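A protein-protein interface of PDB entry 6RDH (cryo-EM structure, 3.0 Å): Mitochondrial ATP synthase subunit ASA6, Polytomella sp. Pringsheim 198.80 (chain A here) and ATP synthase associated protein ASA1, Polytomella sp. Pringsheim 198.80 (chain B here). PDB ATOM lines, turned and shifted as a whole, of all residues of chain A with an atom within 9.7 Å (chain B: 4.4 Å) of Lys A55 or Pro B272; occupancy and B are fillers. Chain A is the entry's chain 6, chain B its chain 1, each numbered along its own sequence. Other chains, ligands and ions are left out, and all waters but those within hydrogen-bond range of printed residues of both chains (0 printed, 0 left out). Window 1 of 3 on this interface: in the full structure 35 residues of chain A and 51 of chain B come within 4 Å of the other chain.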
ATOM      1  N   SER A  31      -6.949  25.648   3.107  1.00  0.00           N
ATOM      2  CA  SER A  31      -6.397  25.645   1.765  1.00  0.00           C
ATOM      3  C   SER A  31      -5.586  24.407   1.450  1.00  0.00           C
ATOM      4  O   SER A  31      -5.333  24.139   0.277  1.00  0.00           O
ATOM      5  CB  SER A  31      -5.530  26.881   1.566  1.00  0.00           C
ATOM      6  OG  SER A  31      -4.410  26.847   2.424  1.00  0.00           O
ATOM      7  N   GLY A  34      -8.048  22.136   0.046  1.00  0.00           N
ATOM      8  CA  GLY A  34      -8.264  22.615  -1.305  1.00  0.00           C
ATOM      9  C   GLY A  34      -7.169  22.190  -2.260  1.00  0.00           C
ATOM     10  O   GLY A  34      -7.448  21.840  -3.405  1.00  0.00           O
ATOM     11  N   ILE A  35      -5.914  22.194  -1.801  1.00  0.00           N
ATOM     12  CA  ILE A  35      -4.806  21.699  -2.617  1.00  0.00           C
ATOM     13  C   ILE A  35      -4.946  20.208  -2.869  1.00  0.00           C
ATOM     14  O   ILE A  35      -4.752  19.739  -3.990  1.00  0.00           O
ATOM     15  CB  ILE A  35      -3.455  22.037  -1.956  1.00  0.00           C
ATOM     16  CG1 ILE A  35      -3.139  23.514  -2.109  1.00  0.00           C
ATOM     17  CG2 ILE A  35      -2.323  21.235  -2.533  1.00  0.00           C
ATOM     18  CD1 ILE A  35      -1.919  23.941  -1.359  1.00  0.00           C
ATOM     19  N   ILE A  36      -5.318  19.453  -1.842  1.00  0.00           N
ATOM     20  CA  ILE A  36      -5.455  18.006  -1.954  1.00  0.00           C
ATOM     21  C   ILE A  36      -6.566  17.646  -2.925  1.00  0.00           C
ATOM     22  O   ILE A  36      -6.376  16.815  -3.820  1.00  0.00           O
ATOM     23  CB  ILE A  36      -5.692  17.405  -0.559  1.00  0.00           C
ATOM     24  CG1 ILE A  36      -4.387  17.376   0.223  1.00  0.00           C
ATOM     25  CG2 ILE A  36      -6.282  16.030  -0.645  1.00  0.00           C
ATOM     26  CD1 ILE A  36      -4.572  17.065   1.655  1.00  0.00           C
ATOM     27  N   SER A  38      -7.894  19.713  -5.304  1.00  0.00           N
ATOM     28  CA  SER A  38      -7.578  20.221  -6.630  1.00  0.00           C
ATOM     29  C   SER A  38      -6.420  19.496  -7.294  1.00  0.00           C
ATOM     30  O   SER A  38      -6.247  19.636  -8.503  1.00  0.00           O
ATOM     31  CB  SER A  38      -7.263  21.709  -6.557  1.00  0.00           C
ATOM     32  OG  SER A  38      -8.401  22.444  -6.157  1.00  0.00           O
ATOM     33  N   VAL A  39      -5.614  18.751  -6.550  1.00  0.00           N
ATOM     34  CA  VAL A  39      -4.600  17.907  -7.171  1.00  0.00           C
ATOM     35  C   VAL A  39      -5.165  16.538  -7.511  1.00  0.00           C
ATOM     36  O   VAL A  39      -4.885  16.004  -8.586  1.00  0.00           O
ATOM     37  CB  VAL A  39      -3.354  17.822  -6.264  1.00  0.00           C
ATOM     38  CG1 VAL A  39      -2.433  16.728  -6.684  1.00  0.00           C
ATOM     39  CG2 VAL A  39      -2.577  19.103  -6.353  1.00  0.00           C
ATOM     40  N   LEU A  47      -1.302  17.940 -15.184  1.00  0.00           N
ATOM     41  CA  LEU A  47      -0.976  18.192 -13.788  1.00  0.00           C
ATOM     42  C   LEU A  47       0.046  19.307 -13.658  1.00  0.00           C
ATOM     43  O   LEU A  47      -0.180  20.276 -12.933  1.00  0.00           O
ATOM     44  CB  LEU A  47      -0.442  16.929 -13.123  1.00  0.00           C
ATOM     45  CG  LEU A  47      -0.044  17.088 -11.659  1.00  0.00           C
ATOM     46  CD1 LEU A  47      -1.269  17.076 -10.798  1.00  0.00           C
ATOM     47  CD2 LEU A  47       0.904  16.006 -11.232  1.00  0.00           C
ATOM     48  N   LEU A  48       1.173  19.194 -14.359  1.00  0.00           N
ATOM     49  CA  LEU A  48       2.233  20.178 -14.190  1.00  0.00           C
ATOM     50  C   LEU A  48       1.894  21.514 -14.828  1.00  0.00           C
ATOM     51  O   LEU A  48       2.471  22.536 -14.457  1.00  0.00           O
ATOM     52  CB  LEU A  48       3.554  19.659 -14.750  1.00  0.00           C
ATOM     53  CG  LEU A  48       4.366  18.745 -13.831  1.00  0.00           C
ATOM     54  CD1 LEU A  48       3.891  17.308 -13.853  1.00  0.00           C
ATOM     55  CD2 LEU A  48       5.839  18.844 -14.136  1.00  0.00           C
ATOM     56  N   SER A  49       0.967  21.539 -15.780  1.00  0.00           N
ATOM     57  CA  SER A  49       0.473  22.826 -16.246  1.00  0.00           C
ATOM     58  C   SER A  49      -0.407  23.479 -15.196  1.00  0.00           C
ATOM     59  O   SER A  49      -0.351  24.698 -15.009  1.00  0.00           O
ATOM     60  CB  SER A  49      -0.302  22.652 -17.547  1.00  0.00           C
ATOM     61  OG  SER A  49      -1.479  21.897 -17.327  1.00  0.00           O
ATOM     62  N   SER A  50      -1.198  22.685 -14.487  1.00  0.00           N
ATOM     63  CA  SER A  50      -2.166  23.206 -13.541  1.00  0.00           C
ATOM     64  C   SER A  50      -1.580  23.508 -12.176  1.00  0.00           C
ATOM     65  O   SER A  50      -2.334  23.900 -11.288  1.00  0.00           O
ATOM     66  CB  SER A  50      -3.313  22.216 -13.371  1.00  0.00           C
ATOM     67  OG  SER A  50      -4.211  22.668 -12.379  1.00  0.00           O
ATOM     68  N   LEU A  51      -0.274  23.343 -11.975  1.00  0.00           N
ATOM     69  CA  LEU A  51       0.263  23.450 -10.625  1.00  0.00           C
ATOM     70  C   LEU A  51       0.350  24.888 -10.147  1.00  0.00           C
ATOM     71  O   LEU A  51       0.169  25.141  -8.955  1.00  0.00           O
ATOM     72  CB  LEU A  51       1.637  22.796 -10.546  1.00  0.00           C
ATOM     73  CG  LEU A  51       1.671  21.286 -10.325  1.00  0.00           C
ATOM     74  CD1 LEU A  51       3.069  20.851  -9.972  1.00  0.00           C
ATOM     75  CD2 LEU A  51       0.697  20.876  -9.250  1.00  0.00           C
ATOM     76  N   LYS A  52       0.609  25.841 -11.045  1.00  0.00           N
ATOM     77  CA  LYS A  52       0.644  27.240 -10.632  1.00  0.00           C
ATOM     78  C   LYS A  52      -0.746  27.764 -10.311  1.00  0.00           C
ATOM     79  O   LYS A  52      -0.888  28.662  -9.479  1.00  0.00           O
ATOM     80  CB  LYS A  52       1.292  28.094 -11.710  1.00  0.00           C
ATOM     81  CG  LYS A  52       2.663  27.612 -12.111  1.00  0.00           C
ATOM     82  CD  LYS A  52       3.334  28.570 -13.075  1.00  0.00           C
ATOM     83  CE  LYS A  52       3.764  29.845 -12.381  1.00  0.00           C
ATOM     84  NZ  LYS A  52       4.643  30.666 -13.254  1.00  0.00           N
ATOM     85  N   THR A  53      -1.778  27.189 -10.924  1.00  0.00           N
ATOM     86  CA  THR A  53      -3.143  27.577 -10.596  1.00  0.00           C
ATOM     87  C   THR A  53      -3.522  27.127  -9.196  1.00  0.00           C
ATOM     88  O   THR A  53      -4.207  27.853  -8.472  1.00  0.00           O
ATOM     89  CB  THR A  53      -4.112  27.000 -11.624  1.00  0.00           C
ATOM     90  OG1 THR A  53      -3.601  27.223 -12.942  1.00  0.00           O
ATOM     91  CG2 THR A  53      -5.466  27.662 -11.509  1.00  0.00           C
ATOM     92  N   ILE A  54      -3.072  25.943  -8.784  1.00  0.00           N
ATOM     93  CA  ILE A  54      -3.365  25.489  -7.429  1.00  0.00           C
ATOM     94  C   ILE A  54      -2.453  26.172  -6.424  1.00  0.00           C
ATOM     95  O   ILE A  54      -2.829  26.356  -5.263  1.00  0.00           O
ATOM     96  CB  ILE A  54      -3.260  23.960  -7.345  1.00  0.00           C
ATOM     97  CG1 ILE A  54      -3.939  23.322  -8.545  1.00  0.00           C
ATOM     98  CG2 ILE A  54      -3.963  23.452  -6.125  1.00  0.00           C
ATOM     99  CD1 ILE A  54      -3.778  21.843  -8.606  1.00  0.00           C
ATOM    100  N   LYS A  55      -1.253  26.563  -6.841  1.00  0.00           N
ATOM    101  CA  LYS A  55      -0.384  27.340  -5.971  1.00  0.00           C
ATOM    102  C   LYS A  55      -0.971  28.716  -5.699  1.00  0.00           C
ATOM    103  O   LYS A  55      -0.902  29.212  -4.572  1.00  0.00           O
ATOM    104  CB  LYS A  55       0.996  27.463  -6.603  1.00  0.00           C
ATOM    105  CG  LYS A  55       1.991  28.277  -5.823  1.00  0.00           C
ATOM    106  CD  LYS A  55       2.634  27.456  -4.739  1.00  0.00           C
ATOM    107  CE  LYS A  55       3.925  28.101  -4.279  1.00  0.00           C
ATOM    108  NZ  LYS A  55       4.741  27.190  -3.432  1.00  0.00           N
ATOM    109  N   ALA A  56      -1.574  29.338  -6.710  1.00  0.00           N
ATOM    110  CA  ALA A  56      -2.152  30.661  -6.538  1.00  0.00           C
ATOM    111  C   ALA A  56      -3.561  30.628  -5.974  1.00  0.00           C
ATOM    112  O   ALA A  56      -4.016  31.637  -5.438  1.00  0.00           O
ATOM    113  CB  ALA A  56      -2.155  31.405  -7.870  1.00  0.00           C
ATOM    114  N   GLN A  57      -4.269  29.505  -6.090  1.00  0.00           N
ATOM    115  CA  GLN A  57      -5.582  29.391  -5.469  1.00  0.00           C
ATOM    116  C   GLN A  57      -5.501  29.256  -3.961  1.00  0.00           C
ATOM    117  O   GLN A  57      -6.487  29.533  -3.276  1.00  0.00           O
ATOM    118  CB  GLN A  57      -6.335  28.181  -6.007  1.00  0.00           C
ATOM    119  CG  GLN A  57      -7.268  28.457  -7.148  1.00  0.00           C
ATOM    120  CD  GLN A  57      -8.123  27.250  -7.463  1.00  0.00           C
ATOM    121  OE1 GLN A  57      -8.177  26.299  -6.684  1.00  0.00           O
ATOM    122  NE2 GLN A  57      -8.790  27.275  -8.609  1.00  0.00           N
ATOM    123  N   ALA A  58      -4.369  28.808  -3.432  1.00  0.00           N
ATOM    124  CA  ALA A  58      -4.215  28.576  -2.006  1.00  0.00           C
ATOM    125  C   ALA A  58      -3.201  29.505  -1.363  1.00  0.00           C
ATOM    126  O   ALA A  58      -2.884  29.334  -0.185  1.00  0.00           O
ATOM    127  CB  ALA A  58      -3.822  27.130  -1.750  1.00  0.00           C
ATOM    128  N   ALA A  59      -2.667  30.460  -2.105  1.00  0.00           N
ATOM    129  CA  ALA A  59      -1.872  31.504  -1.493  1.00  0.00           C
ATOM    130  C   ALA A  59      -2.789  32.433  -0.706  1.00  0.00           C
ATOM    131  O   ALA A  59      -3.897  32.724  -1.159  1.00  0.00           O
ATOM    132  CB  ALA A  59      -1.113  32.288  -2.556  1.00  0.00           C
ATOM    133  N   PRO A  60      -2.367  32.901   0.470  1.00  0.00           N
ATOM    134  CA  PRO A  60      -3.266  33.683   1.324  1.00  0.00           C
ATOM    135  C   PRO A  60      -3.558  35.054   0.745  1.00  0.00           C
ATOM    136  O   PRO A  60      -2.837  35.561  -0.112  1.00  0.00           O
ATOM    137  CB  PRO A  60      -2.486  33.794   2.632  1.00  0.00           C
ATOM    138  CG  PRO A  60      -1.093  33.648   2.237  1.00  0.00           C
ATOM    139  CD  PRO A  60      -1.070  32.678   1.124  1.00  0.00           C
ATOM    140  N   ILE A  61      -4.649  35.653   1.207  1.00  0.00           N
ATOM    141  CA  ILE A  61      -5.047  36.939   0.658  1.00  0.00           C
ATOM    142  C   ILE A  61      -4.251  38.040   1.338  1.00  0.00           C
ATOM    143  O   ILE A  61      -4.250  38.177   2.563  1.00  0.00           O
ATOM    144  CB  ILE A  61      -6.567  37.166   0.771  1.00  0.00           C
ATOM    145  CG1 ILE A  61      -6.909  38.575   0.302  1.00  0.00           C
ATOM    146  CG2 ILE A  61      -7.120  36.904   2.168  1.00  0.00           C
ATOM    147  CD1 ILE A  61      -8.376  38.844   0.149  1.00  0.00           C
ATOM    148  N   THR A 145      10.717  21.086  10.349  1.00  0.00           N
ATOM    149  CA  THR A 145      10.640  20.758   8.917  1.00  0.00           C
ATOM    150  C   THR A 145      11.036  19.310   8.603  1.00  0.00           C
ATOM    151  O   THR A 145      10.686  18.775   7.548  1.00  0.00           O
ATOM    152  CB  THR A 145      11.511  21.752   8.115  1.00  0.00           C
ATOM    153  OG1 THR A 145      11.212  23.084   8.542  1.00  0.00           O
ATOM    154  CG2 THR A 145      11.220  21.717   6.621  1.00  0.00           C
ATOM    155  N   LEU B 268       4.937  19.539  -2.335  1.00  0.00           N
ATOM    156  CA  LEU B 268       5.725  20.674  -2.788  1.00  0.00           C
ATOM    157  C   LEU B 268       4.882  21.898  -3.096  1.00  0.00           C
ATOM    158  O   LEU B 268       5.439  22.955  -3.390  1.00  0.00           O
ATOM    159  CB  LEU B 268       6.537  20.298  -4.025  1.00  0.00           C
ATOM    160  CG  LEU B 268       7.634  19.268  -3.802  1.00  0.00           C
ATOM    161  CD1 LEU B 268       8.300  18.947  -5.098  1.00  0.00           C
ATOM    162  CD2 LEU B 268       8.639  19.779  -2.835  1.00  0.00           C
ATOM    163  N   LEU B 269       3.563  21.773  -3.074  1.00  0.00           N
ATOM    164  CA  LEU B 269       2.730  22.960  -3.091  1.00  0.00           C
ATOM    165  C   LEU B 269       2.569  23.525  -1.697  1.00  0.00           C
ATOM    166  O   LEU B 269       2.465  24.743  -1.536  1.00  0.00           O
ATOM    167  CB  LEU B 269       1.359  22.642  -3.677  1.00  0.00           C
ATOM    168  CG  LEU B 269       1.195  22.622  -5.187  1.00  0.00           C
ATOM    169  CD1 LEU B 269      -0.251  22.403  -5.514  1.00  0.00           C
ATOM    170  CD2 LEU B 269       1.699  23.892  -5.785  1.00  0.00           C
ATOM    171  N   VAL B 270       2.542  22.664  -0.681  1.00  0.00           N
ATOM    172  CA  VAL B 270       2.444  23.161   0.685  1.00  0.00           C
ATOM    173  C   VAL B 270       3.790  23.684   1.165  1.00  0.00           C
ATOM    174  O   VAL B 270       3.903  24.828   1.614  1.00  0.00           O
ATOM    175  CB  VAL B 270       1.894  22.065   1.610  1.00  0.00           C
ATOM    176  CG1 VAL B 270       2.106  22.432   3.047  1.00  0.00           C
ATOM    177  CG2 VAL B 270       0.437  21.870   1.350  1.00  0.00           C
ATOM    178  N   SER B 271       4.836  22.871   1.063  1.00  0.00           N
ATOM    179  CA  SER B 271       6.160  23.228   1.566  1.00  0.00           C
ATOM    180  C   SER B 271       7.196  22.962   0.487  1.00  0.00           C
ATOM    181  O   SER B 271       7.788  21.878   0.439  1.00  0.00           O
ATOM    182  CB  SER B 271       6.500  22.442   2.823  1.00  0.00           C
ATOM    183  OG  SER B 271       6.897  21.135   2.482  1.00  0.00           O
ATOM    184  N   PRO B 272       7.469  23.940  -0.377  1.00  0.00           N
ATOM    185  CA  PRO B 272       8.373  23.714  -1.506  1.00  0.00           C
ATOM    186  C   PRO B 272       9.838  23.638  -1.138  1.00  0.00           C
ATOM    187  O   PRO B 272      10.661  23.399  -2.023  1.00  0.00           O
ATOM    188  CB  PRO B 272       8.109  24.930  -2.390  1.00  0.00           C
ATOM    189  CG  PRO B 272       7.704  25.969  -1.455  1.00  0.00           C
ATOM    190  CD  PRO B 272       6.892  25.288  -0.411  1.00  0.00           C
ATOM    191  N   GLU B 273      10.193  23.821   0.130  1.00  0.00           N
ATOM    192  CA  GLU B 273      11.585  23.720   0.535  1.00  0.00           C
ATOM    193  C   GLU B 273      12.079  22.289   0.541  1.00  0.00           C
ATOM    194  O   GLU B 273      13.290  22.078   0.576  1.00  0.00           O
ATOM    195  CB  GLU B 273      11.782  24.328   1.918  1.00  0.00           C
ATOM    196  CG  GLU B 273      11.137  23.556   3.034  1.00  0.00           C
ATOM    197  CD  GLU B 273       9.808  24.130   3.438  1.00  0.00           C
ATOM    198  OE1 GLU B 273       9.347  25.081   2.781  1.00  0.00           O
ATOM    199  OE2 GLU B 273       9.222  23.629   4.418  1.00  0.00           O
ATOM    200  N   LEU B 274      11.177  21.306   0.474  1.00  0.00           N
ATOM    201  CA  LEU B 274      11.547  19.893   0.516  1.00  0.00           C
ATOM    202  C   LEU B 274      12.347  19.448  -0.693  1.00  0.00           C
ATOM    203  O   LEU B 274      12.958  18.381  -0.650  1.00  0.00           O
ATOM    204  CB  LEU B 274      10.292  19.034   0.627  1.00  0.00           C
ATOM    205  CG  LEU B 274       9.927  18.478   1.994  1.00  0.00           C
ATOM    206  CD1 LEU B 274       9.773  19.577   2.991  1.00  0.00           C
ATOM    207  CD2 LEU B 274       8.638  17.710   1.885  1.00  0.00           C
ATOM    208  N   ALA B 275      12.370  20.234  -1.760  1.00  0.00           N
ATOM    209  CA  ALA B 275      13.135  19.926  -2.955  1.00  0.00           C
ATOM    210  C   ALA B 275      14.608  20.299  -2.847  1.00  0.00           C
ATOM    211  O   ALA B 275      15.278  20.363  -3.876  1.00  0.00           O
ATOM    212  CB  ALA B 275      12.516  20.633  -4.156  1.00  0.00           C
ATOM    213  N   LEU B 351      12.265  27.981  -6.194  1.00  0.00           N
ATOM    214  CA  LEU B 351      11.313  26.910  -5.942  1.00  0.00           C
ATOM    215  C   LEU B 351       9.882  27.386  -5.749  1.00  0.00           C
ATOM    216  O   LEU B 351       9.044  26.593  -5.319  1.00  0.00           O
ATOM    217  CB  LEU B 351      11.738  26.115  -4.712  1.00  0.00           C
ATOM    218  CG  LEU B 351      13.080  25.406  -4.780  1.00  0.00           C
ATOM    219  CD1 LEU B 351      13.374  24.808  -3.450  1.00  0.00           C
ATOM    220  CD2 LEU B 351      13.052  24.339  -5.833  1.00  0.00           C
ATOM    221  N   GLU B 352       9.570  28.645  -6.038  1.00  0.00           N
ATOM    222  CA  GLU B 352       8.170  29.039  -5.979  1.00  0.00           C
ATOM    223  C   GLU B 352       7.398  28.617  -7.219  1.00  0.00           C
ATOM    224  O   GLU B 352       6.165  28.679  -7.208  1.00  0.00           O
ATOM    225  CB  GLU B 352       8.026  30.546  -5.764  1.00  0.00           C
ATOM    226  CG  GLU B 352       8.520  31.023  -4.405  1.00  0.00           C
ATOM    227  CD  GLU B 352       7.659  30.543  -3.244  1.00  0.00           C
ATOM    228  OE1 GLU B 352       8.216  29.945  -2.300  1.00  0.00           O
ATOM    229  OE2 GLU B 352       6.432  30.771  -3.266  1.00  0.00           O
ATOM    230  N   LYS B 530       4.446  27.872   8.793  1.00  0.00           N
ATOM    231  CA  LYS B 530       5.261  28.564   7.805  1.00  0.00           C
ATOM    232  C   LYS B 530       4.759  29.977   7.578  1.00  0.00           C
ATOM    233  O   LYS B 530       5.556  30.914   7.491  1.00  0.00           O
ATOM    234  CB  LYS B 530       5.263  27.788   6.496  1.00  0.00           C
ATOM    235  CG  LYS B 530       6.384  26.784   6.342  1.00  0.00           C
ATOM    236  CD  LYS B 530       6.419  26.241   4.926  1.00  0.00           C
ATOM    237  CE  LYS B 530       6.543  27.374   3.930  1.00  0.00           C
ATOM    238  NZ  LYS B 530       6.609  26.915   2.533  1.00  0.00           N
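Of the 22 printed residues of chain A, 5 touch a printed residue of chain B. Printed residues of chain A that touch a printed residue of chain B: Ile A35, Leu A51, Ile A54, Lys A55 and Thr A145. Among the printed residues, 7 pairs touch across the chains.
The side-chain amino group of Lys A55 is in salt-bridge range of the side-chain carboxylate of Glu B352, 3.96 Å away.
The side-chain amino group (NZ) of Lys B530 lies within salt-bridge range of the side-chain carboxylate (OE1) of Glu B273 (3.3 Å).
Leu B269 touches Ile A35 (CD1 to CG2, 3.8 Å). O of Leu A51 touches CD2 of Leu B269 (3.7 Å). CD1 of Leu B269 touches CB of Ile A54, at 3.9 Å. CB of Lys A55 touches CD2 of Leu B269, 3.7 Å away. NZ of Lys A55 touches CG of Pro B272, 3.8 Å away. Thr A145 touches Glu B273 (CG2 to OE2, 3.5 Å).
Of the printed residues of chain B, Ile A35 touches Leu B269. Leu A47 touches none of the printed residues of chain B. Printed residues of chain B within 4 Å of Leu A51: Leu B269. Of the printed residues of chain B, Ile A54 touches Leu B269. Lys A55 touches just these residues of chain B: Leu B269, Pro B272 and Glu B352. Of the printed residues of chain B, Thr A145 touches Glu B273 (3.5 Å). Leu B269 touches just these residues of chain A: Ile A35, Leu A51, Ile A54 and Lys A55. No residue of chain A comes within 4 Å of Ser B271. Of chain A, only Lys A55 (3.8 Å) comes within 4 Å of Pro B272. Leu B274 touches none of the printed residues of chain A. Glu B352 touches just one residue of chain A: Lys A55. The nearest printed residue of chain B that does not touch Ile A54 is Val B270 (8.0 Å).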
